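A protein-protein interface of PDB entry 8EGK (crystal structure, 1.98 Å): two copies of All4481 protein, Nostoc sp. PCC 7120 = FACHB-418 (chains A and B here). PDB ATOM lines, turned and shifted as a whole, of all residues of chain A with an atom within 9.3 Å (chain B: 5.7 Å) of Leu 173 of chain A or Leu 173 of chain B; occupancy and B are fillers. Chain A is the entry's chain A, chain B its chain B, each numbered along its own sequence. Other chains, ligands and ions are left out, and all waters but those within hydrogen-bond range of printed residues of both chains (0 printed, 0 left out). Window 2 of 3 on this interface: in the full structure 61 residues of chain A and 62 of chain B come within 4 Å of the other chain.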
ATOM      1  N   THR A 167      10.292  14.521 -18.186  1.00  0.00           N
ATOM      2  CA  THR A 167      10.542  15.724 -17.401  1.00  0.00           C
ATOM      3  C   THR A 167      10.690  16.961 -18.277  1.00  0.00           C
ATOM      4  O   THR A 167      10.874  18.063 -17.739  1.00  0.00           O
ATOM      5  CB  THR A 167      11.795  15.563 -16.525  1.00  0.00           C
ATOM      6  OG1 THR A 167      12.970  15.864 -17.289  1.00  0.00           O
ATOM      7  CG2 THR A 167      11.905  14.144 -15.958  1.00  0.00           C
ATOM      8  N   ILE A 168      10.629  16.808 -19.598  1.00  0.00           N
ATOM      9  CA  ILE A 168      10.597  17.938 -20.514  1.00  0.00           C
ATOM     10  C   ILE A 168       9.287  17.919 -21.293  1.00  0.00           C
ATOM     11  O   ILE A 168       8.738  18.975 -21.633  1.00  0.00           O
ATOM     12  CB  ILE A 168      11.798  17.950 -21.479  1.00  0.00           C
ATOM     13  CG1 ILE A 168      13.112  17.659 -20.752  1.00  0.00           C
ATOM     14  CG2 ILE A 168      11.880  19.284 -22.216  1.00  0.00           C
ATOM     15  CD1 ILE A 168      14.027  16.719 -21.508  1.00  0.00           C
ATOM     16  N   ALA A 169       8.775  16.720 -21.592  1.00  0.00           N
ATOM     17  CA  ALA A 169       7.516  16.630 -22.325  1.00  0.00           C
ATOM     18  C   ALA A 169       6.371  17.267 -21.546  1.00  0.00           C
ATOM     19  O   ALA A 169       5.429  17.794 -22.149  1.00  0.00           O
ATOM     20  CB  ALA A 169       7.190  15.169 -22.646  1.00  0.00           C
ATOM     21  N   GLU A 170       6.433  17.234 -20.213  1.00  0.00           N
ATOM     22  CA  GLU A 170       5.401  17.843 -19.388  1.00  0.00           C
ATOM     23  C   GLU A 170       5.829  19.163 -18.766  1.00  0.00           C
ATOM     24  O   GLU A 170       4.968  19.986 -18.441  1.00  0.00           O
ATOM     25  CB  GLU A 170       4.987  16.907 -18.246  1.00  0.00           C
ATOM     26  CG  GLU A 170       4.930  15.436 -18.583  1.00  0.00           C
ATOM     27  CD  GLU A 170       4.608  14.602 -17.358  1.00  0.00           C
ATOM     28  OE1 GLU A 170       3.410  14.420 -17.062  1.00  0.00           O
ATOM     29  OE2 GLU A 170       5.552  14.162 -16.669  1.00  0.00           O
ATOM     30  N   SER A 171       7.130  19.366 -18.578  1.00  0.00           N
ATOM     31  CA  SER A 171       7.669  20.520 -17.875  1.00  0.00           C
ATOM     32  C   SER A 171       6.869  21.782 -18.160  1.00  0.00           C
ATOM     33  O   SER A 171       6.960  22.340 -19.259  1.00  0.00           O
ATOM     34  CB  SER A 171       9.135  20.744 -18.271  1.00  0.00           C
ATOM     35  OG  SER A 171       9.616  21.975 -17.763  1.00  0.00           O
ATOM     36  N   PRO A 172       6.075  22.268 -17.197  1.00  0.00           N
ATOM     37  CA  PRO A 172       5.415  23.569 -17.382  1.00  0.00           C
ATOM     38  C   PRO A 172       6.393  24.727 -17.446  1.00  0.00           C
ATOM     39  O   PRO A 172       5.968  25.872 -17.626  1.00  0.00           O
ATOM     40  CB  PRO A 172       4.503  23.668 -16.150  1.00  0.00           C
ATOM     41  CG  PRO A 172       5.246  22.917 -15.101  1.00  0.00           C
ATOM     42  CD  PRO A 172       5.874  21.745 -15.829  1.00  0.00           C
ATOM     43  N   LEU A 173       7.690  24.454 -17.296  1.00  0.00           N
ATOM     44  CA  LEU A 173       8.714  25.484 -17.427  1.00  0.00           C
ATOM     45  C   LEU A 173       9.086  25.691 -18.892  1.00  0.00           C
ATOM     46  O   LEU A 173       9.176  26.829 -19.362  1.00  0.00           O
ATOM     47  CB  LEU A 173       9.945  25.087 -16.612  1.00  0.00           C
ATOM     48  CG  LEU A 173      10.246  25.790 -15.286  1.00  0.00           C
ATOM     49  CD1 LEU A 173      11.728  25.626 -14.947  1.00  0.00           C
ATOM     50  CD2 LEU A 173       9.871  27.257 -15.298  1.00  0.00           C
ATOM     51  N   ILE A 174       9.297  24.597 -19.626  1.00  0.00           N
ATOM     52  CA  ILE A 174       9.717  24.694 -21.021  1.00  0.00           C
ATOM     53  C   ILE A 174       8.527  24.838 -21.967  1.00  0.00           C
ATOM     54  O   ILE A 174       8.645  25.491 -23.011  1.00  0.00           O
ATOM     55  CB  ILE A 174      10.574  23.475 -21.412  1.00  0.00           C
ATOM     56  CG1 ILE A 174       9.723  22.196 -21.443  1.00  0.00           C
ATOM     57  CG2 ILE A 174      11.747  23.305 -20.450  1.00  0.00           C
ATOM     58  CD1 ILE A 174       9.114  21.881 -22.803  1.00  0.00           C
ATOM     59  N   GLN A 175       7.389  24.233 -21.633  1.00  0.00           N
ATOM     60  CA  GLN A 175       6.214  24.300 -22.501  1.00  0.00           C
ATOM     61  C   GLN A 175       5.824  25.727 -22.862  1.00  0.00           C
ATOM     62  O   GLN A 175       5.662  26.012 -24.059  1.00  0.00           O
ATOM     63  CB  GLN A 175       5.047  23.569 -21.821  1.00  0.00           C
ATOM     64  CG  GLN A 175       5.293  22.082 -21.603  1.00  0.00           C
ATOM     65  CD  GLN A 175       4.509  21.209 -22.564  1.00  0.00           C
ATOM     66  OE1 GLN A 175       4.353  21.543 -23.740  1.00  0.00           O
ATOM     67  NE2 GLN A 175       4.013  20.079 -22.070  1.00  0.00           N
ATOM     68  N   PRO A 176       5.659  26.654 -21.915  1.00  0.00           N
ATOM     69  CA  PRO A 176       5.383  28.045 -22.313  1.00  0.00           C
ATOM     70  C   PRO A 176       6.509  28.656 -23.124  1.00  0.00           C
ATOM     71  O   PRO A 176       6.261  29.551 -23.942  1.00  0.00           O
ATOM     72  CB  PRO A 176       5.195  28.764 -20.969  1.00  0.00           C
ATOM     73  CG  PRO A 176       5.976  27.933 -19.995  1.00  0.00           C
ATOM     74  CD  PRO A 176       5.758  26.511 -20.450  1.00  0.00           C
ATOM     75  N   LEU A 177       7.745  28.192 -22.923  1.00  0.00           N
ATOM     76  CA  LEU A 177       8.871  28.740 -23.672  1.00  0.00           C
ATOM     77  C   LEU A 177       8.823  28.320 -25.135  1.00  0.00           C
ATOM     78  O   LEU A 177       9.246  29.085 -26.009  1.00  0.00           O
ATOM     79  CB  LEU A 177      10.186  28.307 -23.021  1.00  0.00           C
ATOM     80  CG  LEU A 177      10.379  28.808 -21.587  1.00  0.00           C
ATOM     81  CD1 LEU A 177      11.636  28.238 -20.944  1.00  0.00           C
ATOM     82  CD2 LEU A 177      10.401  30.336 -21.550  1.00  0.00           C
ATOM     83  N   ILE A 178       8.312  27.122 -25.425  1.00  0.00           N
ATOM     84  CA  ILE A 178       8.132  26.718 -26.817  1.00  0.00           C
ATOM     85  C   ILE A 178       6.872  27.353 -27.395  1.00  0.00           C
ATOM     86  O   ILE A 178       6.868  27.831 -28.535  1.00  0.00           O
ATOM     87  CB  ILE A 178       8.105  25.179 -26.936  1.00  0.00           C
ATOM     88  CG1 ILE A 178       9.450  24.604 -26.475  1.00  0.00           C
ATOM     89  CG2 ILE A 178       7.777  24.755 -28.368  1.00  0.00           C
ATOM     90  CD1 ILE A 178       9.812  23.258 -27.074  1.00  0.00           C
ATOM     91  N   SER A 179       5.783  27.371 -26.625  1.00  0.00           N
ATOM     92  CA  SER A 179       4.586  28.081 -27.058  1.00  0.00           C
ATOM     93  C   SER A 179       4.892  29.529 -27.418  1.00  0.00           C
ATOM     94  O   SER A 179       4.128  30.151 -28.162  1.00  0.00           O
ATOM     95  CB  SER A 179       3.517  28.017 -25.961  1.00  0.00           C
ATOM     96  OG  SER A 179       3.679  29.062 -25.020  1.00  0.00           O
ATOM     97  N   SER A 180       5.997  30.072 -26.916  1.00  0.00           N
ATOM     98  CA  SER A 180       6.438  31.423 -27.232  1.00  0.00           C
ATOM     99  C   SER A 180       7.516  31.358 -28.309  1.00  0.00           C
ATOM    100  O   SER A 180       8.529  30.670 -28.139  1.00  0.00           O
ATOM    101  CB  SER A 180       6.966  32.121 -25.978  1.00  0.00           C
ATOM    102  OG  SER A 180       7.575  33.358 -26.299  1.00  0.00           O
ATOM    103  N   PHE A 181       7.292  32.070 -29.413  1.00  0.00           N
ATOM    104  CA  PHE A 181       8.195  32.227 -30.551  1.00  0.00           C
ATOM    105  C   PHE A 181       8.170  31.034 -31.501  1.00  0.00           C
ATOM    106  O   PHE A 181       8.954  31.021 -32.458  1.00  0.00           O
ATOM    107  CB  PHE A 181       9.655  32.468 -30.130  1.00  0.00           C
ATOM    108  CG  PHE A 181       9.825  33.572 -29.125  1.00  0.00           C
ATOM    109  CD1 PHE A 181       9.601  34.892 -29.482  1.00  0.00           C
ATOM    110  CD2 PHE A 181      10.213  33.290 -27.823  1.00  0.00           C
ATOM    111  CE1 PHE A 181       9.757  35.910 -28.563  1.00  0.00           C
ATOM    112  CE2 PHE A 181      10.369  34.304 -26.895  1.00  0.00           C
ATOM    113  CZ  PHE A 181      10.141  35.616 -27.267  1.00  0.00           C
ATOM    114  N   SER B 171      13.168  36.181 -18.483  1.00  0.00           N
ATOM    115  CA  SER B 171      12.147  35.185 -18.254  1.00  0.00           C
ATOM    116  C   SER B 171      12.482  34.418 -16.983  1.00  0.00           C
ATOM    117  O   SER B 171      13.628  33.961 -16.835  1.00  0.00           O
ATOM    118  CB  SER B 171      12.022  34.217 -19.434  1.00  0.00           C
ATOM    119  OG  SER B 171      11.133  33.153 -19.133  1.00  0.00           O
ATOM    120  N   PRO B 172      11.528  34.267 -16.057  1.00  0.00           N
ATOM    121  CA  PRO B 172      11.797  33.469 -14.854  1.00  0.00           C
ATOM    122  C   PRO B 172      11.699  31.974 -15.090  1.00  0.00           C
ATOM    123  O   PRO B 172      11.994  31.201 -14.169  1.00  0.00           O
ATOM    124  CB  PRO B 172      10.713  33.943 -13.881  1.00  0.00           C
ATOM    125  CG  PRO B 172       9.546  34.209 -14.782  1.00  0.00           C
ATOM    126  CD  PRO B 172      10.135  34.760 -16.078  1.00  0.00           C
ATOM    127  N   LEU B 173      11.283  31.546 -16.280  1.00  0.00           N
ATOM    128  CA  LEU B 173      11.194  30.132 -16.616  1.00  0.00           C
ATOM    129  C   LEU B 173      12.540  29.536 -17.009  1.00  0.00           C
ATOM    130  O   LEU B 173      12.583  28.378 -17.436  1.00  0.00           O
ATOM    131  CB  LEU B 173      10.196  29.925 -17.761  1.00  0.00           C
ATOM    132  CG  LEU B 173       8.769  30.440 -17.566  1.00  0.00           C
ATOM    133  CD1 LEU B 173       8.165  30.837 -18.909  1.00  0.00           C
ATOM    134  CD2 LEU B 173       7.897  29.402 -16.880  1.00  0.00           C
ATOM    135  N   ILE B 174      13.622  30.296 -16.883  1.00  0.00           N
ATOM    136  CA  ILE B 174      14.954  29.838 -17.265  1.00  0.00           C
ATOM    137  C   ILE B 174      15.791  29.484 -16.045  1.00  0.00           C
ATOM    138  O   ILE B 174      16.394  28.415 -15.987  1.00  0.00           O
ATOM    139  CB  ILE B 174      15.658  30.908 -18.131  1.00  0.00           C
ATOM    140  CG1 ILE B 174      14.818  31.231 -19.370  1.00  0.00           C
ATOM    141  CG2 ILE B 174      17.059  30.447 -18.515  1.00  0.00           C
ATOM    142  CD1 ILE B 174      14.878  30.175 -20.459  1.00  0.00           C
ATOM    143  N   GLN B 175      15.827  30.374 -15.053  1.00  0.00           N
ATOM    144  CA  GLN B 175      16.641  30.127 -13.865  1.00  0.00           C
ATOM    145  C   GLN B 175      16.263  28.834 -13.154  1.00  0.00           C
ATOM    146  O   GLN B 175      17.171  28.059 -12.805  1.00  0.00           O
ATOM    147  CB  GLN B 175      16.542  31.328 -12.919  1.00  0.00           C
ATOM    148  CG  GLN B 175      17.855  31.697 -12.243  1.00  0.00           C
ATOM    149  CD  GLN B 175      18.963  31.993 -13.240  1.00  0.00           C
ATOM    150  OE1 GLN B 175      20.059  31.436 -13.152  1.00  0.00           O
ATOM    151  NE2 GLN B 175      18.678  32.866 -14.201  1.00  0.00           N
ATOM    152  N   PRO B 176      14.984  28.540 -12.894  1.00  0.00           N
ATOM    153  CA  PRO B 176      14.632  27.225 -12.333  1.00  0.00           C
ATOM    154  C   PRO B 176      14.686  26.106 -13.360  1.00  0.00           C
ATOM    155  O   PRO B 176      14.505  24.937 -12.991  1.00  0.00           O
ATOM    156  CB  PRO B 176      13.204  27.440 -11.816  1.00  0.00           C
ATOM    157  CG  PRO B 176      12.634  28.454 -12.753  1.00  0.00           C
ATOM    158  CD  PRO B 176      13.786  29.357 -13.176  1.00  0.00           C
ATOM    159  N   LEU B 177      14.924  26.435 -14.632  1.00  0.00           N
ATOM    160  CA  LEU B 177      15.125  25.425 -15.667  1.00  0.00           C
ATOM    161  C   LEU B 177      16.559  24.912 -15.647  1.00  0.00           C
ATOM    162  O   LEU B 177      16.799  23.705 -15.537  1.00  0.00           O
ATOM    163  CB  LEU B 177      14.786  26.018 -17.033  1.00  0.00           C
ATOM    164  CG  LEU B 177      14.462  25.081 -18.195  1.00  0.00           C
ATOM    165  CD1 LEU B 177      13.972  25.933 -19.365  1.00  0.00           C
ATOM    166  CD2 LEU B 177      15.650  24.235 -18.607  1.00  0.00           C
ATOM    167  N   SER B 180      17.144  22.930 -12.751  1.00  0.00           N
ATOM    168  CA  SER B 180      16.551  21.600 -12.829  1.00  0.00           C
ATOM    169  C   SER B 180      17.601  20.542 -13.136  1.00  0.00           C
ATOM    170  O   SER B 180      17.399  19.365 -12.815  1.00  0.00           O
ATOM    171  CB  SER B 180      15.452  21.574 -13.894  1.00  0.00           C
ATOM    172  OG  SER B 180      15.967  21.180 -15.154  1.00  0.00           O
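Of the 15 printed residues of chain A, 4 touch a printed residue of chain B.
Among the printed residues, 9 pairs touch across the chains.
Among the printed residues, no Asp or Glu carboxylate lies within 4 Å of a Lys or Arg side-chain nitrogen of the other chain.
Leu 173 of chain A touches Pro 176 of chain B, and with the chains exchanged Pro 176 of chain A touches Leu 173 of chain B.
Leu 173 of chain A touches Leu 177 of chain B, and with the chains exchanged Leu 177 of chain A touches Leu 173 of chain B.
Ile 174 of chain A touches Leu 177 of chain B, and with the chains exchanged Leu 177 of chain A touches Ile 174 of chain B.
Leu 177 of chain A touches Ser 171 of chain B, but with the chains exchanged Ser 171 of chain A does not touch Leu 177 of chain B (5.8 Å).
Positions printed for both chains: 171, 172, 173, 174, 175, 176, 177 and 180.
Of the 9 pairs that touch across the chains among the printed residues, 8 have their exchanged pair printed and touching as well.
Leu 173 of chain A touches Leu 173 of chain B.
CD1 of Leu 173 of chain A touches C of Pro 176 of chain B (3.4 Å).
Leu 173 of chain A touches Leu 177 of chain B.
Ile 174 of chain A touches Leu 177 of chain B (CG2 to CD1, 3.6 Å).
Pro 176 of chain A touches Leu 173 of chain B (CG to CD1, 3.8 Å).
Leu 177 of chain A touches Ser 171 of chain B (CD2 to OG, 3.8 Å).
CD2 of Leu 177 of chain A touches CD1 of Leu 173 of chain B (3.5 Å).
CD1 of Leu 177 of chain A touches CD1 of Ile 174 of chain B, 3.8 Å away.
CD1 of Leu 177 of chain A touches CD1 of Leu 177 of chain B, at 3.6 Å.
The side-chain hydroxyl (OG) of Ser 171 of chain A lies close to the backbone NH (N) of Leu 173 of chain A (3.2 Å).
N of Ile 174 of chain A sits at hydrogen-bond distance from OG of Ser 171 of chain A (3.2 Å).
The backbone carbonyl oxygen of Pro 176 of chain A lies within hydrogen-bond range of the side-chain hydroxyl of Ser 179 of chain A (2.8 Å).
The side-chain hydroxyl of Ser 171 of chain B lies close to the backbone NH of Leu 173 of chain B.
The side-chain hydroxyl (OG) of Ser 180 of chain B sits at hydrogen-bond distance from the backbone carbonyl oxygen (O) of Leu 177 of chain B (2.7 Å).
Leu 173 of chain A touches just these residues of chain B: Leu 173, Pro 176 and Leu 177.
Leu 173 of chain B touches three residues of chain A.
Ile 174 of chain B touches just one residue of chain A: Leu 177.
Pro 176 of chain B touches one residue of chain A.
Of the printed residues of chain A, Leu 177 of chain B touches Leu 173, Ile 174 and Leu 177.
Of the printed residues of chain A, Ser 171 of chain B touches Leu 177 (3.8 Å).
Of the printed residues of chain B, Pro 176 of chain A touches Leu 173 (3.8 Å).
Printed residues of chain B within 4 Å of Leu 177 of chain A: Ser 171, Leu 173, Ile 174 and Leu 177.
Of the printed residues of chain B, Ile 174 of chain A touches Leu 177 (3.6 Å).
Glu 170 of chain A touches none of the printed residues of chain B.
Ala 169 of chain A touches none of the printed residues of chain B.
The nearest residue of chain B that does not touch Leu 173 of chain A is Pro 172 of chain B (4.6 Å).
The nearest printed residue of chain B that does not touch Leu 177 of chain A is Pro 172 of chain B (6.8 Å).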
